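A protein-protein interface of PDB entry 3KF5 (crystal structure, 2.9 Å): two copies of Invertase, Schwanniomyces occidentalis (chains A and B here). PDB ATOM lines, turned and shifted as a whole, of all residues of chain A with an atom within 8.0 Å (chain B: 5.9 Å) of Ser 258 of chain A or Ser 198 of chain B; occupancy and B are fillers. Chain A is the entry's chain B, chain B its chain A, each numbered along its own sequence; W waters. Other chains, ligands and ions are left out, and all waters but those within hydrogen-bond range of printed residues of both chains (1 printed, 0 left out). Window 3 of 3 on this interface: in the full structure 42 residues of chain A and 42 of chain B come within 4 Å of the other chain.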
ATOM      1  N   PHE A 197     -29.844  30.683  12.372  1.00  0.00           N
ATOM      2  CA  PHE A 197     -29.517  30.264  13.737  1.00  0.00           C
ATOM      3  C   PHE A 197     -28.360  29.258  13.797  1.00  0.00           C
ATOM      4  O   PHE A 197     -28.364  28.256  13.070  1.00  0.00           O
ATOM      5  CB  PHE A 197     -30.762  29.735  14.469  1.00  0.00           C
ATOM      6  CG  PHE A 197     -30.494  29.297  15.886  1.00  0.00           C
ATOM      7  CD1 PHE A 197     -30.308  30.238  16.899  1.00  0.00           C
ATOM      8  CD2 PHE A 197     -30.419  27.941  16.205  1.00  0.00           C
ATOM      9  CE1 PHE A 197     -30.050  29.839  18.213  1.00  0.00           C
ATOM     10  CE2 PHE A 197     -30.164  27.523  17.517  1.00  0.00           C
ATOM     11  CZ  PHE A 197     -29.979  28.477  18.523  1.00  0.00           C
ATOM     12  N   SER A 199     -25.898  27.311  16.806  1.00  0.00           N
ATOM     13  CA  SER A 199     -25.511  27.036  18.189  1.00  0.00           C
ATOM     14  C   SER A 199     -25.281  25.533  18.416  1.00  0.00           C
ATOM     15  O   SER A 199     -25.263  24.754  17.458  1.00  0.00           O
ATOM     16  CB  SER A 199     -26.577  27.577  19.147  1.00  0.00           C
ATOM     17  OG  SER A 199     -26.003  27.957  20.379  1.00  0.00           O
ATOM     18  N   GLY A 200     -25.088  25.137  19.676  1.00  0.00           N
ATOM     19  CA  GLY A 200     -24.915  23.725  20.047  1.00  0.00           C
ATOM     20  C   GLY A 200     -23.711  22.994  19.462  1.00  0.00           C
ATOM     21  O   GLY A 200     -22.708  23.608  19.112  1.00  0.00           O
ATOM     22  N   PHE A 244     -32.769  22.953  21.518  1.00  0.00           N
ATOM     23  CA  PHE A 244     -32.616  24.220  22.230  1.00  0.00           C
ATOM     24  C   PHE A 244     -33.979  24.697  22.711  1.00  0.00           C
ATOM     25  O   PHE A 244     -34.981  24.531  22.011  1.00  0.00           O
ATOM     26  CB  PHE A 244     -31.995  25.280  21.320  1.00  0.00           C
ATOM     27  CG  PHE A 244     -30.782  24.803  20.558  1.00  0.00           C
ATOM     28  CD1 PHE A 244     -29.501  25.048  21.040  1.00  0.00           C
ATOM     29  CD2 PHE A 244     -30.922  24.117  19.353  1.00  0.00           C
ATOM     30  CE1 PHE A 244     -28.385  24.613  20.337  1.00  0.00           C
ATOM     31  CE2 PHE A 244     -29.809  23.675  18.646  1.00  0.00           C
ATOM     32  CZ  PHE A 244     -28.540  23.924  19.140  1.00  0.00           C
ATOM     33  N   VAL A 245     -34.016  25.296  23.899  1.00  0.00           N
ATOM     34  CA  VAL A 245     -35.271  25.760  24.495  1.00  0.00           C
ATOM     35  C   VAL A 245     -35.292  27.287  24.565  1.00  0.00           C
ATOM     36  O   VAL A 245     -34.397  27.895  25.157  1.00  0.00           O
ATOM     37  CB  VAL A 245     -35.476  25.153  25.907  1.00  0.00           C
ATOM     38  CG1 VAL A 245     -36.712  25.735  26.595  1.00  0.00           C
ATOM     39  CG2 VAL A 245     -35.563  23.631  25.824  1.00  0.00           C
ATOM     40  N   PRO A 255     -33.012  31.415  22.118  1.00  0.00           N
ATOM     41  CA  PRO A 255     -32.934  30.428  23.200  1.00  0.00           C
ATOM     42  C   PRO A 255     -32.742  31.050  24.585  1.00  0.00           C
ATOM     43  O   PRO A 255     -32.104  32.097  24.707  1.00  0.00           O
ATOM     44  CB  PRO A 255     -31.714  29.598  22.819  1.00  0.00           C
ATOM     45  CG  PRO A 255     -30.869  30.517  22.013  1.00  0.00           C
ATOM     46  CD  PRO A 255     -31.813  31.390  21.259  1.00  0.00           C
ATOM     47  N   ASP A 256     -33.293  30.398  25.611  1.00  0.00           N
ATOM     48  CA  ASP A 256     -33.188  30.857  27.000  1.00  0.00           C
ATOM     49  C   ASP A 256     -31.758  30.810  27.516  1.00  0.00           C
ATOM     50  O   ASP A 256     -31.366  31.612  28.358  1.00  0.00           O
ATOM     51  CB  ASP A 256     -34.089  30.026  27.918  1.00  0.00           C
ATOM     52  CG  ASP A 256     -35.573  30.266  27.671  1.00  0.00           C
ATOM     53  OD1 ASP A 256     -35.934  31.263  27.010  1.00  0.00           O
ATOM     54  OD2 ASP A 256     -36.387  29.448  28.147  1.00  0.00           O
ATOM     55  N   ASP A 257     -30.987  29.854  27.016  1.00  0.00           N
ATOM     56  CA  ASP A 257     -29.573  29.745  27.350  1.00  0.00           C
ATOM     57  C   ASP A 257     -28.758  29.361  26.114  1.00  0.00           C
ATOM     58  O   ASP A 257     -29.289  29.322  24.999  1.00  0.00           O
ATOM     59  CB  ASP A 257     -29.341  28.758  28.516  1.00  0.00           C
ATOM     60  CG  ASP A 257     -30.112  27.440  28.362  1.00  0.00           C
ATOM     61  OD1 ASP A 257     -30.789  27.050  29.338  1.00  0.00           O
ATOM     62  OD2 ASP A 257     -30.040  26.793  27.288  1.00  0.00           O
ATOM     63  N   SER A 258     -27.471  29.093  26.321  1.00  0.00           N
ATOM     64  CA  SER A 258     -26.576  28.672  25.251  1.00  0.00           C
ATOM     65  C   SER A 258     -25.911  27.332  25.606  1.00  0.00           C
ATOM     66  O   SER A 258     -24.703  27.140  25.393  1.00  0.00           O
ATOM     67  CB  SER A 258     -25.531  29.756  24.988  1.00  0.00           C
ATOM     68  OG  SER A 258     -24.783  30.037  26.160  1.00  0.00           O
ATOM     69  N   GLN A 259     -26.707  26.412  26.153  1.00  0.00           N
ATOM     70  CA  GLN A 259     -26.214  25.080  26.523  1.00  0.00           C
ATOM     71  C   GLN A 259     -26.578  24.029  25.475  1.00  0.00           C
ATOM     72  O   GLN A 259     -27.593  24.141  24.798  1.00  0.00           O
ATOM     73  CB  GLN A 259     -26.718  24.657  27.915  1.00  0.00           C
ATOM     74  CG  GLN A 259     -28.178  24.207  27.963  1.00  0.00           C
ATOM     75  CD  GLN A 259     -28.580  23.654  29.314  1.00  0.00           C
ATOM     76  OE1 GLN A 259     -28.187  22.547  29.685  1.00  0.00           O
ATOM     77  NE2 GLN A 259     -29.383  24.415  30.052  1.00  0.00           N
ATOM     78  N   THR A 260     -25.743  23.010  25.354  1.00  0.00           N
ATOM     79  CA  THR A 260     -25.988  21.925  24.416  1.00  0.00           C
ATOM     80  C   THR A 260     -26.645  20.754  25.156  1.00  0.00           C
ATOM     81  O   THR A 260     -26.188  20.354  26.224  1.00  0.00           O
ATOM     82  CB  THR A 260     -24.666  21.493  23.740  1.00  0.00           C
ATOM     83  OG1 THR A 260     -24.058  22.648  23.160  1.00  0.00           O
ATOM     84  CG2 THR A 260     -24.901  20.492  22.638  1.00  0.00           C
ATOM     85  N   ARG A 261     -27.731  20.232  24.599  1.00  0.00           N
ATOM     86  CA  ARG A 261     -28.400  19.064  25.160  1.00  0.00           C
ATOM     87  C   ARG A 261     -28.847  18.152  24.024  1.00  0.00           C
ATOM     88  O   ARG A 261     -29.307  18.625  22.980  1.00  0.00           O
ATOM     89  CB  ARG A 261     -29.623  19.461  25.995  1.00  0.00           C
ATOM     90  CG  ARG A 261     -29.366  20.432  27.127  1.00  0.00           C
ATOM     91  CD  ARG A 261     -30.571  20.493  28.044  1.00  0.00           C
ATOM     92  NE  ARG A 261     -30.893  21.861  28.453  1.00  0.00           N
ATOM     93  CZ  ARG A 261     -32.027  22.491  28.164  1.00  0.00           C
ATOM     94  NH1 ARG A 261     -32.969  21.887  27.469  1.00  0.00           N
ATOM     95  NH2 ARG A 261     -32.226  23.730  28.577  1.00  0.00           N
ATOM     96  N   GLU B 177     -24.436  25.978  40.237  1.00  0.00           N
ATOM     97  CA  GLU B 177     -25.178  27.065  39.600  1.00  0.00           C
ATOM     98  C   GLU B 177     -24.858  27.183  38.109  1.00  0.00           C
ATOM     99  O   GLU B 177     -25.445  28.009  37.402  1.00  0.00           O
ATOM    100  CB  GLU B 177     -24.886  28.386  40.299  1.00  0.00           C
ATOM    101  CG  GLU B 177     -25.538  28.533  41.651  1.00  0.00           C
ATOM    102  CD  GLU B 177     -25.406  29.933  42.193  1.00  0.00           C
ATOM    103  OE1 GLU B 177     -25.934  30.871  41.561  1.00  0.00           O
ATOM    104  OE2 GLU B 177     -24.777  30.099  43.256  1.00  0.00           O
ATOM    105  N   TYR B 178     -23.928  26.347  37.645  1.00  0.00           N
ATOM    106  CA  TYR B 178     -23.421  26.374  36.271  1.00  0.00           C
ATOM    107  C   TYR B 178     -22.882  27.754  35.865  1.00  0.00           C
ATOM    108  O   TYR B 178     -23.141  28.226  34.757  1.00  0.00           O
ATOM    109  CB  TYR B 178     -24.486  25.893  35.278  1.00  0.00           C
ATOM    110  CG  TYR B 178     -25.032  24.513  35.551  1.00  0.00           C
ATOM    111  CD1 TYR B 178     -26.314  24.347  36.074  1.00  0.00           C
ATOM    112  CD2 TYR B 178     -24.279  23.367  35.268  1.00  0.00           C
ATOM    113  CE1 TYR B 178     -26.836  23.070  36.320  1.00  0.00           C
ATOM    114  CE2 TYR B 178     -24.786  22.086  35.509  1.00  0.00           C
ATOM    115  CZ  TYR B 178     -26.067  21.947  36.038  1.00  0.00           C
ATOM    116  OH  TYR B 178     -26.595  20.699  36.289  1.00  0.00           O
ATOM    117  N   LYS B 179     -22.136  28.397  36.763  1.00  0.00           N
ATOM    118  CA  LYS B 179     -21.513  29.686  36.457  1.00  0.00           C
ATOM    119  C   LYS B 179     -20.002  29.630  36.678  1.00  0.00           C
ATOM    120  O   LYS B 179     -19.544  29.222  37.750  1.00  0.00           O
ATOM    121  CB  LYS B 179     -22.102  30.807  37.325  1.00  0.00           C
ATOM    122  CG  LYS B 179     -23.610  30.717  37.611  1.00  0.00           C
ATOM    123  CD  LYS B 179     -24.447  31.663  36.760  1.00  0.00           C
ATOM    124  CE  LYS B 179     -24.813  32.946  37.512  1.00  0.00           C
ATOM    125  NZ  LYS B 179     -25.731  32.720  38.659  1.00  0.00           N
ATOM    126  N   ILE B 180     -19.231  30.019  35.661  1.00  0.00           N
ATOM    127  CA  ILE B 180     -17.833  30.392  35.878  1.00  0.00           C
ATOM    128  C   ILE B 180     -17.851  31.845  36.321  1.00  0.00           C
ATOM    129  O   ILE B 180     -18.305  32.724  35.577  1.00  0.00           O
ATOM    130  CB  ILE B 180     -16.964  30.271  34.618  1.00  0.00           C
ATOM    131  CG1 ILE B 180     -16.832  28.812  34.190  1.00  0.00           C
ATOM    132  CG2 ILE B 180     -15.574  30.837  34.888  1.00  0.00           C
ATOM    133  CD1 ILE B 180     -16.757  28.628  32.696  1.00  0.00           C
ATOM    134  N   ASN B 196     -20.354  36.755  35.327  1.00  0.00           N
ATOM    135  CA  ASN B 196     -20.730  35.355  35.387  1.00  0.00           C
ATOM    136  C   ASN B 196     -20.805  34.821  33.961  1.00  0.00           C
ATOM    137  O   ASN B 196     -21.358  35.483  33.084  1.00  0.00           O
ATOM    138  CB  ASN B 196     -22.115  35.216  36.033  1.00  0.00           C
ATOM    139  CG  ASN B 196     -22.123  35.533  37.529  1.00  0.00           C
ATOM    140  OD1 ASN B 196     -21.123  35.353  38.232  1.00  0.00           O
ATOM    141  ND2 ASN B 196     -23.278  36.001  38.020  1.00  0.00           N
ATOM    142  N   PHE B 197     -20.266  33.626  33.725  1.00  0.00           N
ATOM    143  CA  PHE B 197     -20.357  33.009  32.400  1.00  0.00           C
ATOM    144  C   PHE B 197     -20.949  31.596  32.440  1.00  0.00           C
ATOM    145  O   PHE B 197     -20.530  30.762  33.251  1.00  0.00           O
ATOM    146  CB  PHE B 197     -18.992  33.021  31.702  1.00  0.00           C
ATOM    147  CG  PHE B 197     -19.008  32.409  30.326  1.00  0.00           C
ATOM    148  CD1 PHE B 197     -19.557  33.103  29.246  1.00  0.00           C
ATOM    149  CD2 PHE B 197     -18.474  31.128  30.107  1.00  0.00           C
ATOM    150  CE1 PHE B 197     -19.580  32.533  27.974  1.00  0.00           C
ATOM    151  CE2 PHE B 197     -18.490  30.550  28.841  1.00  0.00           C
ATOM    152  CZ  PHE B 197     -19.043  31.249  27.774  1.00  0.00           C
ATOM    153  N   SER B 198     -21.919  31.342  31.555  1.00  0.00           N
ATOM    154  CA  SER B 198     -22.645  30.066  31.506  1.00  0.00           C
ATOM    155  C   SER B 198     -22.963  29.623  30.085  1.00  0.00           C
ATOM    156  O   SER B 198     -23.825  30.204  29.427  1.00  0.00           O
ATOM    157  CB  SER B 198     -23.957  30.164  32.290  1.00  0.00           C
ATOM    158  OG  SER B 198     -23.729  30.536  33.635  1.00  0.00           O
ATOM    159  N   SER B 199     -22.290  28.576  29.621  1.00  0.00           N
ATOM    160  CA  SER B 199     -22.521  28.056  28.277  1.00  0.00           C
ATOM    161  C   SER B 199     -22.091  26.594  28.157  1.00  0.00           C
ATOM    162  O   SER B 199     -21.799  25.947  29.170  1.00  0.00           O
ATOM    163  CB  SER B 199     -21.771  28.906  27.261  1.00  0.00           C
ATOM    164  OG  SER B 199     -22.407  28.816  26.009  1.00  0.00           O
ATOM    165  N   GLY B 200     -22.064  26.072  26.927  1.00  0.00           N
ATOM    166  CA  GLY B 200     -21.549  24.720  26.651  1.00  0.00           C
ATOM    167  C   GLY B 200     -22.329  23.564  27.261  1.00  0.00           C
ATOM    168  O   GLY B 200     -23.534  23.680  27.514  1.00  0.00           O
ATOM    169  N   TYR B 202     -23.536  21.418  30.139  1.00  0.00           N
ATOM    170  CA  TYR B 202     -23.712  21.637  31.581  1.00  0.00           C
ATOM    171  C   TYR B 202     -23.326  20.407  32.402  1.00  0.00           C
ATOM    172  O   TYR B 202     -22.526  20.511  33.342  1.00  0.00           O
ATOM    173  CB  TYR B 202     -25.152  22.054  31.913  1.00  0.00           C
ATOM    174  CG  TYR B 202     -25.463  23.531  31.769  1.00  0.00           C
ATOM    175  CD1 TYR B 202     -24.621  24.388  31.056  1.00  0.00           C
ATOM    176  CD2 TYR B 202     -26.626  24.068  32.324  1.00  0.00           C
ATOM    177  CE1 TYR B 202     -24.920  25.744  30.917  1.00  0.00           C
ATOM    178  CE2 TYR B 202     -26.933  25.425  32.190  1.00  0.00           C
ATOM    179  CZ  TYR B 202     -26.076  26.254  31.484  1.00  0.00           C
ATOM    180  OH  TYR B 202     -26.373  27.591  31.349  1.00  0.00           O
ATOM    181  N   TYR B 206     -20.134  22.512  37.065  1.00  0.00           N
ATOM    182  CA  TYR B 206     -18.942  23.164  36.528  1.00  0.00           C
ATOM    183  C   TYR B 206     -17.799  22.924  37.513  1.00  0.00           C
ATOM    184  O   TYR B 206     -17.986  23.048  38.726  1.00  0.00           O
ATOM    185  CB  TYR B 206     -19.157  24.679  36.401  1.00  0.00           C
ATOM    186  CG  TYR B 206     -19.876  25.196  35.158  1.00  0.00           C
ATOM    187  CD1 TYR B 206     -20.786  24.408  34.452  1.00  0.00           C
ATOM    188  CD2 TYR B 206     -19.671  26.501  34.724  1.00  0.00           C
ATOM    189  CE1 TYR B 206     -21.449  24.902  33.332  1.00  0.00           C
ATOM    190  CE2 TYR B 206     -20.322  27.001  33.613  1.00  0.00           C
ATOM    191  CZ  TYR B 206     -21.213  26.200  32.922  1.00  0.00           C
ATOM    192  OH  TYR B 206     -21.869  26.703  31.820  1.00  0.00           O
ATOM    193  N   SER B 258     -21.484  30.220  19.991  1.00  0.00           N
ATOM    194  CA  SER B 258     -22.122  29.535  21.102  1.00  0.00           C
ATOM    195  C   SER B 258     -22.134  28.022  20.859  1.00  0.00           C
ATOM    196  O   SER B 258     -23.141  27.350  21.116  1.00  0.00           O
ATOM    197  CB  SER B 258     -23.542  30.065  21.282  1.00  0.00           C
ATOM    198  OG  SER B 258     -24.302  29.873  20.097  1.00  0.00           O
ATOM    199  N   THR B 260     -20.410  24.084  21.383  1.00  0.00           N
ATOM    200  CA  THR B 260     -19.749  23.294  22.411  1.00  0.00           C
ATOM    201  C   THR B 260     -18.664  22.453  21.759  1.00  0.00           C
ATOM    202  O   THR B 260     -18.913  21.799  20.738  1.00  0.00           O
ATOM    203  CB  THR B 260     -20.757  22.396  23.147  1.00  0.00           C
ATOM    204  OG1 THR B 260     -21.819  23.207  23.670  1.00  0.00           O
ATOM    205  CG2 THR B 260     -20.091  21.661  24.297  1.00  0.00           C
HETATM  206  O   HOH W   1     -26.143  21.193  29.061  1.00  0.00           O
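Ser 199 of chain A touches Ser 258 of chain B, and with the chains exchanged Ser 258 of chain A touches Ser 199 of chain B. Gly 200 of chain A touches Ser 258 of chain B, and with the chains exchanged Ser 258 of chain A touches Gly 200 of chain B. Gly 200 of chain A touches Thr 260 of chain B, and with the chains exchanged Thr 260 of chain A touches Gly 200 of chain B. Thr 260 of chain A touches its own counterpart, Thr 260 of chain B. Of the 10 pairs that touch across the chains among the printed residues, 7 have their exchanged pair printed and touching as well.
Printed residues of chain B within 4 Å of Ser 199 of chain A: Ser 258 (2.6 Å). Of chain B, only Ser 198 (3.4 Å), Ser 199 (2.7 Å) and Gly 200 (3.2 Å) come within 4 Å of Ser 258 of chain A. Of the printed residues of chain B, Gln 259 of chain A touches Gly 200 (3.2 Å) and Tyr 202 (3.4 Å). Asn 196 of chain B touches none of the printed residues of chain A. Phe 197 of chain B touches none of the printed residues of chain A. Ser 198 of chain B touches just one residue of chain A: Ser 258. The nearest printed residue of chain A that does not touch Ser 198 of chain B is Asp 257 of chain A (5.8 Å).
Among the printed residues, pairs that only touch across the chains: Gln 259 of chain A with Gly 200 of chain B and Gln 259 of chain A with Tyr 202 of chain B.
O of Ser 198 of chain B sits at hydrogen-bond distance from OG of Ser 258 of chain A (3.4 Å). The side-chain hydroxyl (OG) of Ser 199 of chain B sits at hydrogen-bond distance from the side-chain hydroxyl (OG) of Ser 258 of chain A, 2.7 Å away. The backbone carbonyl oxygen (O) of Ser 258 of chain A lies within hydrogen-bond range of the backbone NH (N) of Gly 200 of chain B (3.2 Å). The backbone NH of Thr 260 of chain A lies within hydrogen-bond range of the backbone carbonyl oxygen of Gly 200 of chain B, at 3.2 Å. The side-chain hydroxyl (OG) of Ser 258 of chain B lies within hydrogen-bond range of the side-chain hydroxyl (OG) of Ser 199 of chain A. The backbone NH of Gly 200 of chain A is in hydrogen-bond range of the backbone carbonyl oxygen of Ser 258 of chain B (3.3 Å). The backbone carbonyl oxygen (O) of Gly 200 of chain A sits at hydrogen-bond distance from the backbone NH (N) of Thr 260 of chain B (3.3 Å). OG1 of Thr 260 of chain B lies close to OG1 of Thr 260 of chain A (2.4 Å).
The backbone carbonyl oxygen (O) of Tyr 178 of chain B is in hydrogen-bond range of the side-chain hydroxyl (OG) of Ser 198 of chain B. The side-chain hydroxyl (OH) of Tyr 206 of chain B sits at hydrogen-bond distance from the backbone carbonyl oxygen (O) of Ser 199 of chain B, 2.8 Å away. NE2 of Gln 259 of chain A is in hydrogen-bond range of OD1 of Asp 257 of chain A, 3.1 Å away. NE of Arg 261 of chain A sits close to OE1 of Gln 259 of chain A, at 3.1 Å.
Water W1 lies within hydrogen-bond range of the side-chain amide oxygen of Gln 259 of chain A (2.5 Å), the backbone NH of Tyr 202 of chain B (2.8 Å) and the backbone carbonyl oxygen of Thr 260 of chain A (3.0 Å).
Hydrophobic or aromatic side chains of chain B that line the printed part of chain A: Tyr 202. Of the 12 printed residues of chain A, 5 touch a printed residue of chain B. Among the printed residues, no Asp or Glu carboxylate lies within 4 Å of a Lys or Arg side-chain nitrogen of the other chain.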
